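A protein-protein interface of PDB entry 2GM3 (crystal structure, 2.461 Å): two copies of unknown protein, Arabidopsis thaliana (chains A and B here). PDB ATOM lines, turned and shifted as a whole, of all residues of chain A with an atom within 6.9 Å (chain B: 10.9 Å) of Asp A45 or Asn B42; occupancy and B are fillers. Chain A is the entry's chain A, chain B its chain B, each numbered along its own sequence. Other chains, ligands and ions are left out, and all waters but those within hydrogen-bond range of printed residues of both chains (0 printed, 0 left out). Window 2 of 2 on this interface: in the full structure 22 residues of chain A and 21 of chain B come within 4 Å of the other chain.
Ile A38 touches Phe B46, and with the chains exchanged Phe A46 touches Ile B38.
Asn A42 touches its own counterpart, Asn B42.
Asn A42 touches Asp B45, and with the chains exchanged Asp A45 touches Asn B42.
Of the 10 pairs that touch across the chains among the printed residues, 5 have their exchanged pair printed and touching as well.
Pro A5 touches just one residue of chain B: Arg B40 (3.4 Å).
Of chain B, only Lys B37 (2.5 Å) and Arg B40 (3.1 Å) come within 4 Å of Thr A6.
Of the printed residues of chain B, Ile A38 touches Phe B46 (3.7 Å).
Printed residues of chain B within 4 Å of Asn A42: Asn B42 (3.2 Å) and Asp B45 (2.8 Å).
No residue of chain B comes within 4 Å of Thr A43.
No residue of chain B comes within 4 Å of Ser A44.
Of the printed residues of chain B, Asp A45 touches Arg B40 and Asn B42.
Of the printed residues of chain A, Ile B38 touches Phe A46 (3.6 Å).
Printed residues of chain A within 4 Å of Arg B40: Pro A5 (3.4 Å), Thr A6 (3.1 Å) and Asp A45 (2.8 Å).
Printed residues of chain A within 4 Å of Asp B45: Asn A42 (2.8 Å).
The nearest residue of chain B that does not touch Asp A45 is Ser B41 (4.4 Å).
OG1 of Thr A6 lies within hydrogen-bond range of O of Lys B37 (2.5 Å).
The side-chain hydroxyl (OG1) of Thr A6 is in hydrogen-bond range of the guanidinium group (NH1) of Arg B40, at 3.1 Å.
The side-chain amide nitrogen of Asn A42 lies close to the side-chain amide nitrogen of Asn B42 (3.3 Å).
ND2 of Asn A42 is in hydrogen-bond range of OD1 of Asp B45, at 2.8 Å.
OD1 of Asp A45 lies within salt-bridge range of NE of Arg B40 (2.8 Å).
The side-chain carboxylate of Asp A45 lies close to the side-chain amide nitrogen of Asn B42, 3.4 Å away.
The backbone nitrogen of Pro A5 sits close to the guanidinium group of Arg B40, at 3.4 Å.
Among the printed residues, merely in contact across the chains: Phe A46 with Ile B38 (3.6 Å), Ile A38 with Phe B46 (3.7 Å) and Phe A46 with Lys B37 (3.7 Å).
N of Thr A6 is in hydrogen-bond range of O of Asp A45 (2.8 Å).
O of Thr A6 sits at hydrogen-bond distance from N of Lys A47, at 2.8 Å.
The backbone NH of Thr B6 sits at hydrogen-bond distance from the backbone carbonyl oxygen of Asp B45, 2.8 Å away.
N of Arg B40 lies within hydrogen-bond range of O of Leu B35, 2.9 Å away.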
ATOM      1  N   PRO A   5      24.734   4.280 -16.615  1.00  0.00           N
ATOM      2  CA  PRO A   5      23.672   4.962 -17.355  1.00  0.00           C
ATOM      3  C   PRO A   5      22.875   5.827 -16.409  1.00  0.00           C
ATOM      4  O   PRO A   5      22.485   5.373 -15.324  1.00  0.00           O
ATOM      5  CB  PRO A   5      22.806   3.817 -17.935  1.00  0.00           C
ATOM      6  CG  PRO A   5      23.178   2.620 -17.195  1.00  0.00           C
ATOM      7  CD  PRO A   5      24.591   2.816 -16.693  1.00  0.00           C
ATOM      8  N   THR A   6      22.666   7.078 -16.809  1.00  0.00           N
ATOM      9  CA  THR A   6      22.071   8.056 -15.935  1.00  0.00           C
ATOM     10  C   THR A   6      20.578   7.830 -15.886  1.00  0.00           C
ATOM     11  O   THR A   6      19.912   7.781 -16.931  1.00  0.00           O
ATOM     12  CB  THR A   6      22.428   9.452 -16.394  1.00  0.00           C
ATOM     13  OG1 THR A   6      23.811   9.676 -16.112  1.00  0.00           O
ATOM     14  CG2 THR A   6      21.604  10.484 -15.669  1.00  0.00           C
ATOM     15  N   LYS A   7      20.050   7.668 -14.677  1.00  0.00           N
ATOM     16  CA  LYS A   7      18.595   7.465 -14.521  1.00  0.00           C
ATOM     17  C   LYS A   7      17.906   8.799 -14.416  1.00  0.00           C
ATOM     18  O   LYS A   7      18.098   9.551 -13.474  1.00  0.00           O
ATOM     19  CB  LYS A   7      18.233   6.579 -13.315  1.00  0.00           C
ATOM     20  CG  LYS A   7      18.912   5.186 -13.277  1.00  0.00           C
ATOM     21  CD  LYS A   7      18.784   4.590 -11.876  1.00  0.00           C
ATOM     22  CE  LYS A   7      20.078   3.881 -11.433  1.00  0.00           C
ATOM     23  NZ  LYS A   7      20.355   4.070  -9.956  1.00  0.00           N
ATOM     24  N   VAL A   8      17.090   9.086 -15.407  1.00  0.00           N
ATOM     25  CA  VAL A   8      16.359  10.313 -15.472  1.00  0.00           C
ATOM     26  C   VAL A   8      14.888  10.027 -15.163  1.00  0.00           C
ATOM     27  O   VAL A   8      14.186   9.422 -15.986  1.00  0.00           O
ATOM     28  CB  VAL A   8      16.471  10.886 -16.882  1.00  0.00           C
ATOM     29  CG1 VAL A   8      15.841  12.286 -16.952  1.00  0.00           C
ATOM     30  CG2 VAL A   8      17.920  10.910 -17.321  1.00  0.00           C
ATOM     31  N   ILE A  38      19.672  16.680 -23.549  1.00  0.00           N
ATOM     32  CA  ILE A  38      20.452  15.866 -22.597  1.00  0.00           C
ATOM     33  C   ILE A  38      20.814  14.471 -23.121  1.00  0.00           C
ATOM     34  O   ILE A  38      21.979  14.106 -23.135  1.00  0.00           O
ATOM     35  CB  ILE A  38      19.777  15.781 -21.180  1.00  0.00           C
ATOM     36  CG1 ILE A  38      19.426  17.183 -20.647  1.00  0.00           C
ATOM     37  CG2 ILE A  38      20.615  14.939 -20.165  1.00  0.00           C
ATOM     38  CD1 ILE A  38      20.435  17.780 -19.735  1.00  0.00           C
ATOM     39  N   VAL A  39      19.822  13.702 -23.551  1.00  0.00           N
ATOM     40  CA  VAL A  39      20.069  12.364 -24.074  1.00  0.00           C
ATOM     41  C   VAL A  39      20.803  12.484 -25.405  1.00  0.00           C
ATOM     42  O   VAL A  39      21.813  11.808 -25.617  1.00  0.00           O
ATOM     43  CB  VAL A  39      18.751  11.577 -24.259  1.00  0.00           C
ATOM     44  CG1 VAL A  39      19.023  10.223 -24.925  1.00  0.00           C
ATOM     45  CG2 VAL A  39      18.009  11.412 -22.926  1.00  0.00           C
ATOM     46  N   SER A  41      22.015  11.950 -29.084  1.00  0.00           N
ATOM     47  CA  SER A  41      22.168  10.649 -29.751  1.00  0.00           C
ATOM     48  C   SER A  41      22.697   9.559 -28.806  1.00  0.00           C
ATOM     49  O   SER A  41      22.777   8.394 -29.182  1.00  0.00           O
ATOM     50  CB  SER A  41      23.091  10.789 -30.944  1.00  0.00           C
ATOM     51  OG  SER A  41      24.399  11.065 -30.482  1.00  0.00           O
ATOM     52  N   ASN A  42      23.027   9.938 -27.575  1.00  0.00           N
ATOM     53  CA  ASN A  42      23.654   9.012 -26.629  1.00  0.00           C
ATOM     54  C   ASN A  42      22.643   8.227 -25.837  1.00  0.00           C
ATOM     55  O   ASN A  42      22.573   8.323 -24.620  1.00  0.00           O
ATOM     56  CB  ASN A  42      24.604   9.765 -25.712  1.00  0.00           C
ATOM     57  CG  ASN A  42      25.761  10.350 -26.468  1.00  0.00           C
ATOM     58  OD1 ASN A  42      26.433   9.639 -27.238  1.00  0.00           O
ATOM     59  ND2 ASN A  42      25.985  11.653 -26.302  1.00  0.00           N
ATOM     60  N   THR A  43      21.879   7.414 -26.552  1.00  0.00           N
ATOM     61  CA  THR A  43      20.679   6.812 -26.004  1.00  0.00           C
ATOM     62  C   THR A  43      20.950   5.668 -25.042  1.00  0.00           C
ATOM     63  O   THR A  43      20.063   5.275 -24.290  1.00  0.00           O
ATOM     64  CB  THR A  43      19.718   6.391 -27.129  1.00  0.00           C
ATOM     65  OG1 THR A  43      20.456   5.694 -28.131  1.00  0.00           O
ATOM     66  CG2 THR A  43      19.089   7.632 -27.779  1.00  0.00           C
ATOM     67  N   SER A  44      22.164   5.136 -25.050  1.00  0.00           N
ATOM     68  CA  SER A  44      22.524   4.121 -24.059  1.00  0.00           C
ATOM     69  C   SER A  44      23.142   4.690 -22.781  1.00  0.00           C
ATOM     70  O   SER A  44      23.347   3.951 -21.810  1.00  0.00           O
ATOM     71  CB  SER A  44      23.369   3.043 -24.693  1.00  0.00           C
ATOM     72  OG  SER A  44      22.530   2.377 -25.610  1.00  0.00           O
ATOM     73  N   ASP A  45      23.390   6.001 -22.773  1.00  0.00           N
ATOM     74  CA  ASP A  45      23.988   6.662 -21.621  1.00  0.00           C
ATOM     75  C   ASP A  45      22.927   7.114 -20.607  1.00  0.00           C
ATOM     76  O   ASP A  45      23.242   7.510 -19.497  1.00  0.00           O
ATOM     77  CB  ASP A  45      24.907   7.797 -22.098  1.00  0.00           C
ATOM     78  CG  ASP A  45      26.260   7.275 -22.623  1.00  0.00           C
ATOM     79  OD1 ASP A  45      27.264   7.349 -21.870  1.00  0.00           O
ATOM     80  OD2 ASP A  45      26.342   6.771 -23.776  1.00  0.00           O
ATOM     81  N   PHE A  46      21.662   7.013 -21.002  1.00  0.00           N
ATOM     82  CA  PHE A  46      20.536   7.435 -20.177  1.00  0.00           C
ATOM     83  C   PHE A  46      19.424   6.391 -20.135  1.00  0.00           C
ATOM     84  O   PHE A  46      19.194   5.682 -21.113  1.00  0.00           O
ATOM     85  CB  PHE A  46      19.981   8.778 -20.691  1.00  0.00           C
ATOM     86  CG  PHE A  46      20.967   9.901 -20.583  1.00  0.00           C
ATOM     87  CD1 PHE A  46      21.903  10.122 -21.591  1.00  0.00           C
ATOM     88  CD2 PHE A  46      20.993  10.698 -19.456  1.00  0.00           C
ATOM     89  CE1 PHE A  46      22.830  11.132 -21.474  1.00  0.00           C
ATOM     90  CE2 PHE A  46      21.910  11.700 -19.325  1.00  0.00           C
ATOM     91  CZ  PHE A  46      22.836  11.939 -20.337  1.00  0.00           C
ATOM     92  N   LYS A  47      18.730   6.333 -19.007  1.00  0.00           N
ATOM     93  CA  LYS A  47      17.534   5.525 -18.854  1.00  0.00           C
ATOM     94  C   LYS A  47      16.408   6.415 -18.302  1.00  0.00           C
ATOM     95  O   LYS A  47      16.586   7.114 -17.319  1.00  0.00           O
ATOM     96  CB  LYS A  47      17.829   4.354 -17.904  1.00  0.00           C
ATOM     97  CG  LYS A  47      16.634   3.466 -17.645  1.00  0.00           C
ATOM     98  CD  LYS A  47      16.989   2.188 -16.930  1.00  0.00           C
ATOM     99  CE  LYS A  47      15.724   1.371 -16.700  1.00  0.00           C
ATOM    100  NZ  LYS A  47      16.015  -0.109 -16.643  1.00  0.00           N
ATOM    101  N   PRO B   5      26.095  20.993 -29.600  1.00  0.00           N
ATOM    102  CA  PRO B   5      26.701  20.815 -28.277  1.00  0.00           C
ATOM    103  C   PRO B   5      25.861  21.570 -27.244  1.00  0.00           C
ATOM    104  O   PRO B   5      25.635  22.768 -27.377  1.00  0.00           O
ATOM    105  CB  PRO B   5      28.100  21.466 -28.415  1.00  0.00           C
ATOM    106  CG  PRO B   5      28.280  21.723 -29.869  1.00  0.00           C
ATOM    107  CD  PRO B   5      26.911  21.856 -30.470  1.00  0.00           C
ATOM    108  N   THR B   6      25.418  20.877 -26.214  1.00  0.00           N
ATOM    109  CA  THR B   6      24.577  21.470 -25.232  1.00  0.00           C
ATOM    110  C   THR B   6      25.393  22.382 -24.318  1.00  0.00           C
ATOM    111  O   THR B   6      26.350  21.948 -23.665  1.00  0.00           O
ATOM    112  CB  THR B   6      23.808  20.383 -24.463  1.00  0.00           C
ATOM    113  OG1 THR B   6      23.025  19.624 -25.392  1.00  0.00           O
ATOM    114  CG2 THR B   6      22.889  20.990 -23.412  1.00  0.00           C
ATOM    115  N   LYS B   7      25.010  23.659 -24.295  1.00  0.00           N
ATOM    116  CA  LYS B   7      25.709  24.656 -23.513  1.00  0.00           C
ATOM    117  C   LYS B   7      25.089  24.696 -22.112  1.00  0.00           C
ATOM    118  O   LYS B   7      23.905  25.005 -21.928  1.00  0.00           O
ATOM    119  CB  LYS B   7      25.677  26.006 -24.226  1.00  0.00           C
ATOM    120  CG  LYS B   7      26.569  26.026 -25.464  1.00  0.00           C
ATOM    121  CD  LYS B   7      26.413  27.297 -26.306  1.00  0.00           C
ATOM    122  CE  LYS B   7      25.110  27.292 -27.133  1.00  0.00           C
ATOM    123  NZ  LYS B   7      25.019  28.485 -28.069  1.00  0.00           N
ATOM    124  N   VAL B   8      25.903  24.332 -21.132  1.00  0.00           N
ATOM    125  CA  VAL B   8      25.456  24.229 -19.756  1.00  0.00           C
ATOM    126  C   VAL B   8      26.092  25.361 -18.961  1.00  0.00           C
ATOM    127  O   VAL B   8      27.307  25.390 -18.787  1.00  0.00           O
ATOM    128  CB  VAL B   8      25.901  22.883 -19.147  1.00  0.00           C
ATOM    129  CG1 VAL B   8      25.603  22.827 -17.666  1.00  0.00           C
ATOM    130  CG2 VAL B   8      25.268  21.728 -19.906  1.00  0.00           C
ATOM    131  N   TRP B  33      28.353  16.832 -10.108  1.00  0.00           N
ATOM    132  CA  TRP B  33      27.258  15.956 -10.443  1.00  0.00           C
ATOM    133  C   TRP B  33      26.964  16.075 -11.940  1.00  0.00           C
ATOM    134  O   TRP B  33      26.797  15.064 -12.625  1.00  0.00           O
ATOM    135  CB  TRP B  33      26.015  16.223  -9.603  1.00  0.00           C
ATOM    136  CG  TRP B  33      24.911  15.327 -10.026  1.00  0.00           C
ATOM    137  CD1 TRP B  33      24.626  14.078  -9.536  1.00  0.00           C
ATOM    138  CD2 TRP B  33      23.974  15.580 -11.074  1.00  0.00           C
ATOM    139  NE1 TRP B  33      23.544  13.561 -10.196  1.00  0.00           N
ATOM    140  CE2 TRP B  33      23.126  14.457 -11.150  1.00  0.00           C
ATOM    141  CE3 TRP B  33      23.740  16.668 -11.924  1.00  0.00           C
ATOM    142  CZ2 TRP B  33      22.059  14.381 -12.055  1.00  0.00           C
ATOM    143  CZ3 TRP B  33      22.681  16.600 -12.839  1.00  0.00           C
ATOM    144  CH2 TRP B  33      21.859  15.459 -12.893  1.00  0.00           C
ATOM    145  N   THR B  34      26.956  17.307 -12.444  1.00  0.00           N
ATOM    146  CA  THR B  34      26.669  17.542 -13.838  1.00  0.00           C
ATOM    147  C   THR B  34      27.655  16.814 -14.734  1.00  0.00           C
ATOM    148  O   THR B  34      27.262  16.164 -15.710  1.00  0.00           O
ATOM    149  CB  THR B  34      26.697  19.012 -14.170  1.00  0.00           C
ATOM    150  OG1 THR B  34      25.672  19.664 -13.430  1.00  0.00           O
ATOM    151  CG2 THR B  34      26.410  19.230 -15.632  1.00  0.00           C
ATOM    152  N   LEU B  35      28.940  16.900 -14.412  1.00  0.00           N
ATOM    153  CA  LEU B  35      29.931  16.121 -15.156  1.00  0.00           C
ATOM    154  C   LEU B  35      29.746  14.602 -15.037  1.00  0.00           C
ATOM    155  O   LEU B  35      29.843  13.907 -16.036  1.00  0.00           O
ATOM    156  CB  LEU B  35      31.365  16.539 -14.825  1.00  0.00           C
ATOM    157  CG  LEU B  35      31.808  18.009 -14.974  1.00  0.00           C
ATOM    158  CD1 LEU B  35      33.191  18.163 -14.433  1.00  0.00           C
ATOM    159  CD2 LEU B  35      31.739  18.533 -16.403  1.00  0.00           C
ATOM    160  N   GLU B  36      29.472  14.098 -13.838  1.00  0.00           N
ATOM    161  CA  GLU B  36      29.263  12.672 -13.624  1.00  0.00           C
ATOM    162  C   GLU B  36      28.041  12.174 -14.374  1.00  0.00           C
ATOM    163  O   GLU B  36      28.135  11.227 -15.137  1.00  0.00           O
ATOM    164  CB  GLU B  36      28.984  12.400 -12.163  1.00  0.00           C
ATOM    165  CG  GLU B  36      30.101  12.016 -11.312  1.00  0.00           C
ATOM    166  CD  GLU B  36      29.651  12.012  -9.860  1.00  0.00           C
ATOM    167  OE1 GLU B  36      29.053  10.994  -9.418  1.00  0.00           O
ATOM    168  OE2 GLU B  36      29.882  13.040  -9.175  1.00  0.00           O
ATOM    169  N   LYS B  37      26.898  12.812 -14.141  1.00  0.00           N
ATOM    170  CA  LYS B  37      25.644  12.218 -14.534  1.00  0.00           C
ATOM    171  C   LYS B  37      25.068  12.756 -15.850  1.00  0.00           C
ATOM    172  O   LYS B  37      24.328  12.058 -16.530  1.00  0.00           O
ATOM    173  CB  LYS B  37      24.694  12.250 -13.355  1.00  0.00           C
ATOM    174  CG  LYS B  37      25.309  11.606 -12.130  1.00  0.00           C
ATOM    175  CD  LYS B  37      25.590  10.138 -12.412  1.00  0.00           C
ATOM    176  CE  LYS B  37      25.710   9.341 -11.127  1.00  0.00           C
ATOM    177  NZ  LYS B  37      25.977   7.915 -11.439  1.00  0.00           N
ATOM    178  N   ILE B  38      25.473  13.954 -16.247  1.00  0.00           N
ATOM    179  CA  ILE B  38      24.967  14.548 -17.481  1.00  0.00           C
ATOM    180  C   ILE B  38      25.994  14.445 -18.602  1.00  0.00           C
ATOM    181  O   ILE B  38      25.699  13.944 -19.684  1.00  0.00           O
ATOM    182  CB  ILE B  38      24.581  16.046 -17.282  1.00  0.00           C
ATOM    183  CG1 ILE B  38      23.488  16.201 -16.194  1.00  0.00           C
ATOM    184  CG2 ILE B  38      24.249  16.733 -18.647  1.00  0.00           C
ATOM    185  CD1 ILE B  38      22.174  15.530 -16.511  1.00  0.00           C
ATOM    186  N   VAL B  39      27.192  14.959 -18.359  1.00  0.00           N
ATOM    187  CA  VAL B  39      28.218  14.972 -19.389  1.00  0.00           C
ATOM    188  C   VAL B  39      28.736  13.544 -19.588  1.00  0.00           C
ATOM    189  O   VAL B  39      28.978  13.116 -20.716  1.00  0.00           O
ATOM    190  CB  VAL B  39      29.387  15.933 -19.035  1.00  0.00           C
ATOM    191  CG1 VAL B  39      30.556  15.785 -20.045  1.00  0.00           C
ATOM    192  CG2 VAL B  39      28.892  17.373 -18.979  1.00  0.00           C
ATOM    193  N   ARG B  40      28.866  12.810 -18.481  1.00  0.00           N
ATOM    194  CA  ARG B  40      29.410  11.439 -18.477  1.00  0.00           C
ATOM    195  C   ARG B  40      30.697  11.413 -19.299  1.00  0.00           C
ATOM    196  O   ARG B  40      31.495  12.358 -19.227  1.00  0.00           O
ATOM    197  CB  ARG B  40      28.418  10.384 -19.013  1.00  0.00           C
ATOM    198  CG  ARG B  40      27.010  10.534 -18.494  1.00  0.00           C
ATOM    199  CD  ARG B  40      26.037   9.590 -19.221  1.00  0.00           C
ATOM    200  NE  ARG B  40      26.546   8.224 -19.291  1.00  0.00           N
ATOM    201  CZ  ARG B  40      26.411   7.305 -18.335  1.00  0.00           C
ATOM    202  NH1 ARG B  40      25.776   7.583 -17.210  1.00  0.00           N
ATOM    203  NH2 ARG B  40      26.905   6.101 -18.517  1.00  0.00           N
ATOM    204  N   SER B  41      30.881  10.367 -20.099  1.00  0.00           N
ATOM    205  CA  SER B  41      32.025  10.317 -20.985  1.00  0.00           C
ATOM    206  C   SER B  41      31.798  11.060 -22.306  1.00  0.00           C
ATOM    207  O   SER B  41      32.706  11.137 -23.118  1.00  0.00           O
ATOM    208  CB  SER B  41      32.468   8.865 -21.249  1.00  0.00           C
ATOM    209  OG  SER B  41      31.530   8.189 -22.073  1.00  0.00           O
ATOM    210  N   ASN B  42      30.605  11.611 -22.520  1.00  0.00           N
ATOM    211  CA  ASN B  42      30.278  12.293 -23.790  1.00  0.00           C
ATOM    212  C   ASN B  42      30.705  13.751 -23.785  1.00  0.00           C
ATOM    213  O   ASN B  42      29.906  14.680 -23.841  1.00  0.00           O
ATOM    214  CB  ASN B  42      28.787  12.136 -24.132  1.00  0.00           C
ATOM    215  CG  ASN B  42      28.399  10.701 -24.342  1.00  0.00           C
ATOM    216  OD1 ASN B  42      29.071   9.961 -25.086  1.00  0.00           O
ATOM    217  ND2 ASN B  42      27.328  10.271 -23.675  1.00  0.00           N
ATOM    218  N   THR B  43      32.002  13.937 -23.728  1.00  0.00           N
ATOM    219  CA  THR B  43      32.574  15.230 -23.412  1.00  0.00           C
ATOM    220  C   THR B  43      32.519  16.254 -24.549  1.00  0.00           C
ATOM    221  O   THR B  43      32.727  17.446 -24.342  1.00  0.00           O
ATOM    222  CB  THR B  43      33.995  15.038 -22.924  1.00  0.00           C
ATOM    223  OG1 THR B  43      34.520  16.321 -22.616  1.00  0.00           O
ATOM    224  CG2 THR B  43      34.849  14.357 -23.987  1.00  0.00           C
ATOM    225  N   SER B  44      32.238  15.795 -25.754  1.00  0.00           N
ATOM    226  CA  SER B  44      32.091  16.723 -26.866  1.00  0.00           C
ATOM    227  C   SER B  44      30.632  17.111 -27.105  1.00  0.00           C
ATOM    228  O   SER B  44      30.357  17.977 -27.926  1.00  0.00           O
ATOM    229  CB  SER B  44      32.718  16.156 -28.131  1.00  0.00           C
ATOM    230  OG  SER B  44      32.366  14.801 -28.261  1.00  0.00           O
ATOM    231  N   ASP B  45      29.705  16.480 -26.383  1.00  0.00           N
ATOM    232  CA  ASP B  45      28.282  16.766 -26.525  1.00  0.00           C
ATOM    233  C   ASP B  45      27.843  17.964 -25.665  1.00  0.00           C
ATOM    234  O   ASP B  45      26.724  18.465 -25.799  1.00  0.00           O
ATOM    235  CB  ASP B  45      27.452  15.536 -26.164  1.00  0.00           C
ATOM    236  CG  ASP B  45      27.424  14.486 -27.277  1.00  0.00           C
ATOM    237  OD1 ASP B  45      26.317  14.064 -27.676  1.00  0.00           O
ATOM    238  OD2 ASP B  45      28.493  14.060 -27.759  1.00  0.00           O
ATOM    239  N   PHE B  46      28.751  18.422 -24.802  1.00  0.00           N
ATOM    240  CA  PHE B  46      28.475  19.473 -23.833  1.00  0.00           C
ATOM    241  C   PHE B  46      29.577  20.511 -23.799  1.00  0.00           C
ATOM    242  O   PHE B  46      30.744  20.213 -24.066  1.00  0.00           O
ATOM    243  CB  PHE B  46      28.256  18.849 -22.447  1.00  0.00           C
ATOM    244  CG  PHE B  46      27.021  18.006 -22.389  1.00  0.00           C
ATOM    245  CD1 PHE B  46      27.084  16.628 -22.610  1.00  0.00           C
ATOM    246  CD2 PHE B  46      25.781  18.599 -22.220  1.00  0.00           C
ATOM    247  CE1 PHE B  46      25.926  15.843 -22.616  1.00  0.00           C
ATOM    248  CE2 PHE B  46      24.636  17.816 -22.222  1.00  0.00           C
ATOM    249  CZ  PHE B  46      24.720  16.421 -22.415  1.00  0.00           C
ATOM    250  N   LYS B  47      29.184  21.741 -23.502  1.00  0.00           N
ATOM    251  CA  LYS B  47      30.108  22.839 -23.294  1.00  0.00           C
ATOM    252  C   LYS B  47      29.693  23.545 -22.009  1.00  0.00           C
ATOM    253  O   LYS B  47      28.535  23.917 -21.847  1.00  0.00           O
ATOM    254  CB  LYS B  47      30.061  23.820 -24.463  1.00  0.00           C
ATOM    255  CG  LYS B  47      31.211  24.824 -24.380  1.00  0.00           C
ATOM    256  CD  LYS B  47      31.106  25.983 -25.349  1.00  0.00           C
ATOM    257  CE  LYS B  47      32.330  26.866 -25.185  1.00  0.00           C
ATOM    258  NZ  LYS B  47      32.383  27.940 -26.201  1.00  0.00           N
ATOM    259  N   ILE B  48      30.631  23.700 -21.092  1.00  0.00           N
ATOM    260  CA  ILE B  48      30.324  24.264 -19.798  1.00  0.00           C
ATOM    261  C   ILE B  48      30.651  25.741 -19.830  1.00  0.00           C
ATOM    262  O   ILE B  48      31.733  26.153 -20.252  1.00  0.00           O
ATOM    263  CB  ILE B  48      31.095  23.557 -18.669  1.00  0.00           C
ATOM    264  CG1 ILE B  48      31.144  22.037 -18.899  1.00  0.00           C
ATOM    265  CG2 ILE B  48      30.477  23.870 -17.316  1.00  0.00           C
ATOM    266  CD1 ILE B  48      29.782  21.355 -18.980  1.00  0.00           C
ATOM    267  N   CYS B  96      37.324  20.843 -15.937  1.00  0.00           N
ATOM    268  CA  CYS B  96      36.889  20.635 -17.317  1.00  0.00           C
ATOM    269  C   CYS B  96      37.993  20.145 -18.223  1.00  0.00           C
ATOM    270  O   CYS B  96      37.774  19.249 -19.045  1.00  0.00           O
ATOM    271  CB  CYS B  96      36.387  21.930 -17.918  1.00  0.00           C
ATOM    272  SG  CYS B  96      34.883  22.458 -17.219  1.00  0.00           S
ATOM    273  N   ILE B  99      39.023  16.324 -17.769  1.00  0.00           N
ATOM    274  CA  ILE B  99      38.203  15.300 -18.417  1.00  0.00           C
ATOM    275  C   ILE B  99      37.919  15.654 -19.879  1.00  0.00           C
ATOM    276  O   ILE B  99      37.265  14.902 -20.594  1.00  0.00           O
ATOM    277  CB  ILE B  99      36.872  14.976 -17.640  1.00  0.00           C
ATOM    278  CG1 ILE B  99      35.756  15.932 -18.016  1.00  0.00           C
ATOM    279  CG2 ILE B  99      37.079  14.967 -16.118  1.00  0.00           C
ATOM    280  CD1 ILE B  99      34.453  15.538 -17.415  1.00  0.00           C
ATOM    281  N   GLY B 100      38.408  16.809 -20.309  1.00  0.00           N
ATOM    282  CA  GLY B 100      38.347  17.189 -21.708  1.00  0.00           C
ATOM    283  C   GLY B 100      37.064  17.821 -22.194  1.00  0.00           C
ATOM    284  O   GLY B 100      36.796  17.810 -23.390  1.00  0.00           O
ATOM    285  N   VAL B 101      36.255  18.373 -21.285  1.00  0.00           N
ATOM    286  CA  VAL B 101      35.093  19.148 -21.734  1.00  0.00           C
ATOM    287  C   VAL B 101      35.465  20.573 -22.024  1.00  0.00           C
ATOM    288  O   VAL B 101      36.147  21.206 -21.233  1.00  0.00           O
ATOM    289  CB  VAL B 101      33.858  19.199 -20.765  1.00  0.00           C
ATOM    290  CG1 VAL B 101      32.881  18.088 -21.043  1.00  0.00           C
ATOM    291  CG2 VAL B 101      34.261  19.265 -19.288  1.00  0.00           C
ATOM    292  N   GLY B 102      34.972  21.082 -23.148  1.00  0.00           N
ATOM    293  CA  GLY B 102      35.157  22.484 -23.503  1.00  0.00           C
ATOM    294  C   GLY B 102      34.445  23.353 -22.487  1.00  0.00           C
ATOM    295  O   GLY B 102      33.368  23.015 -22.004  1.00  0.00           O
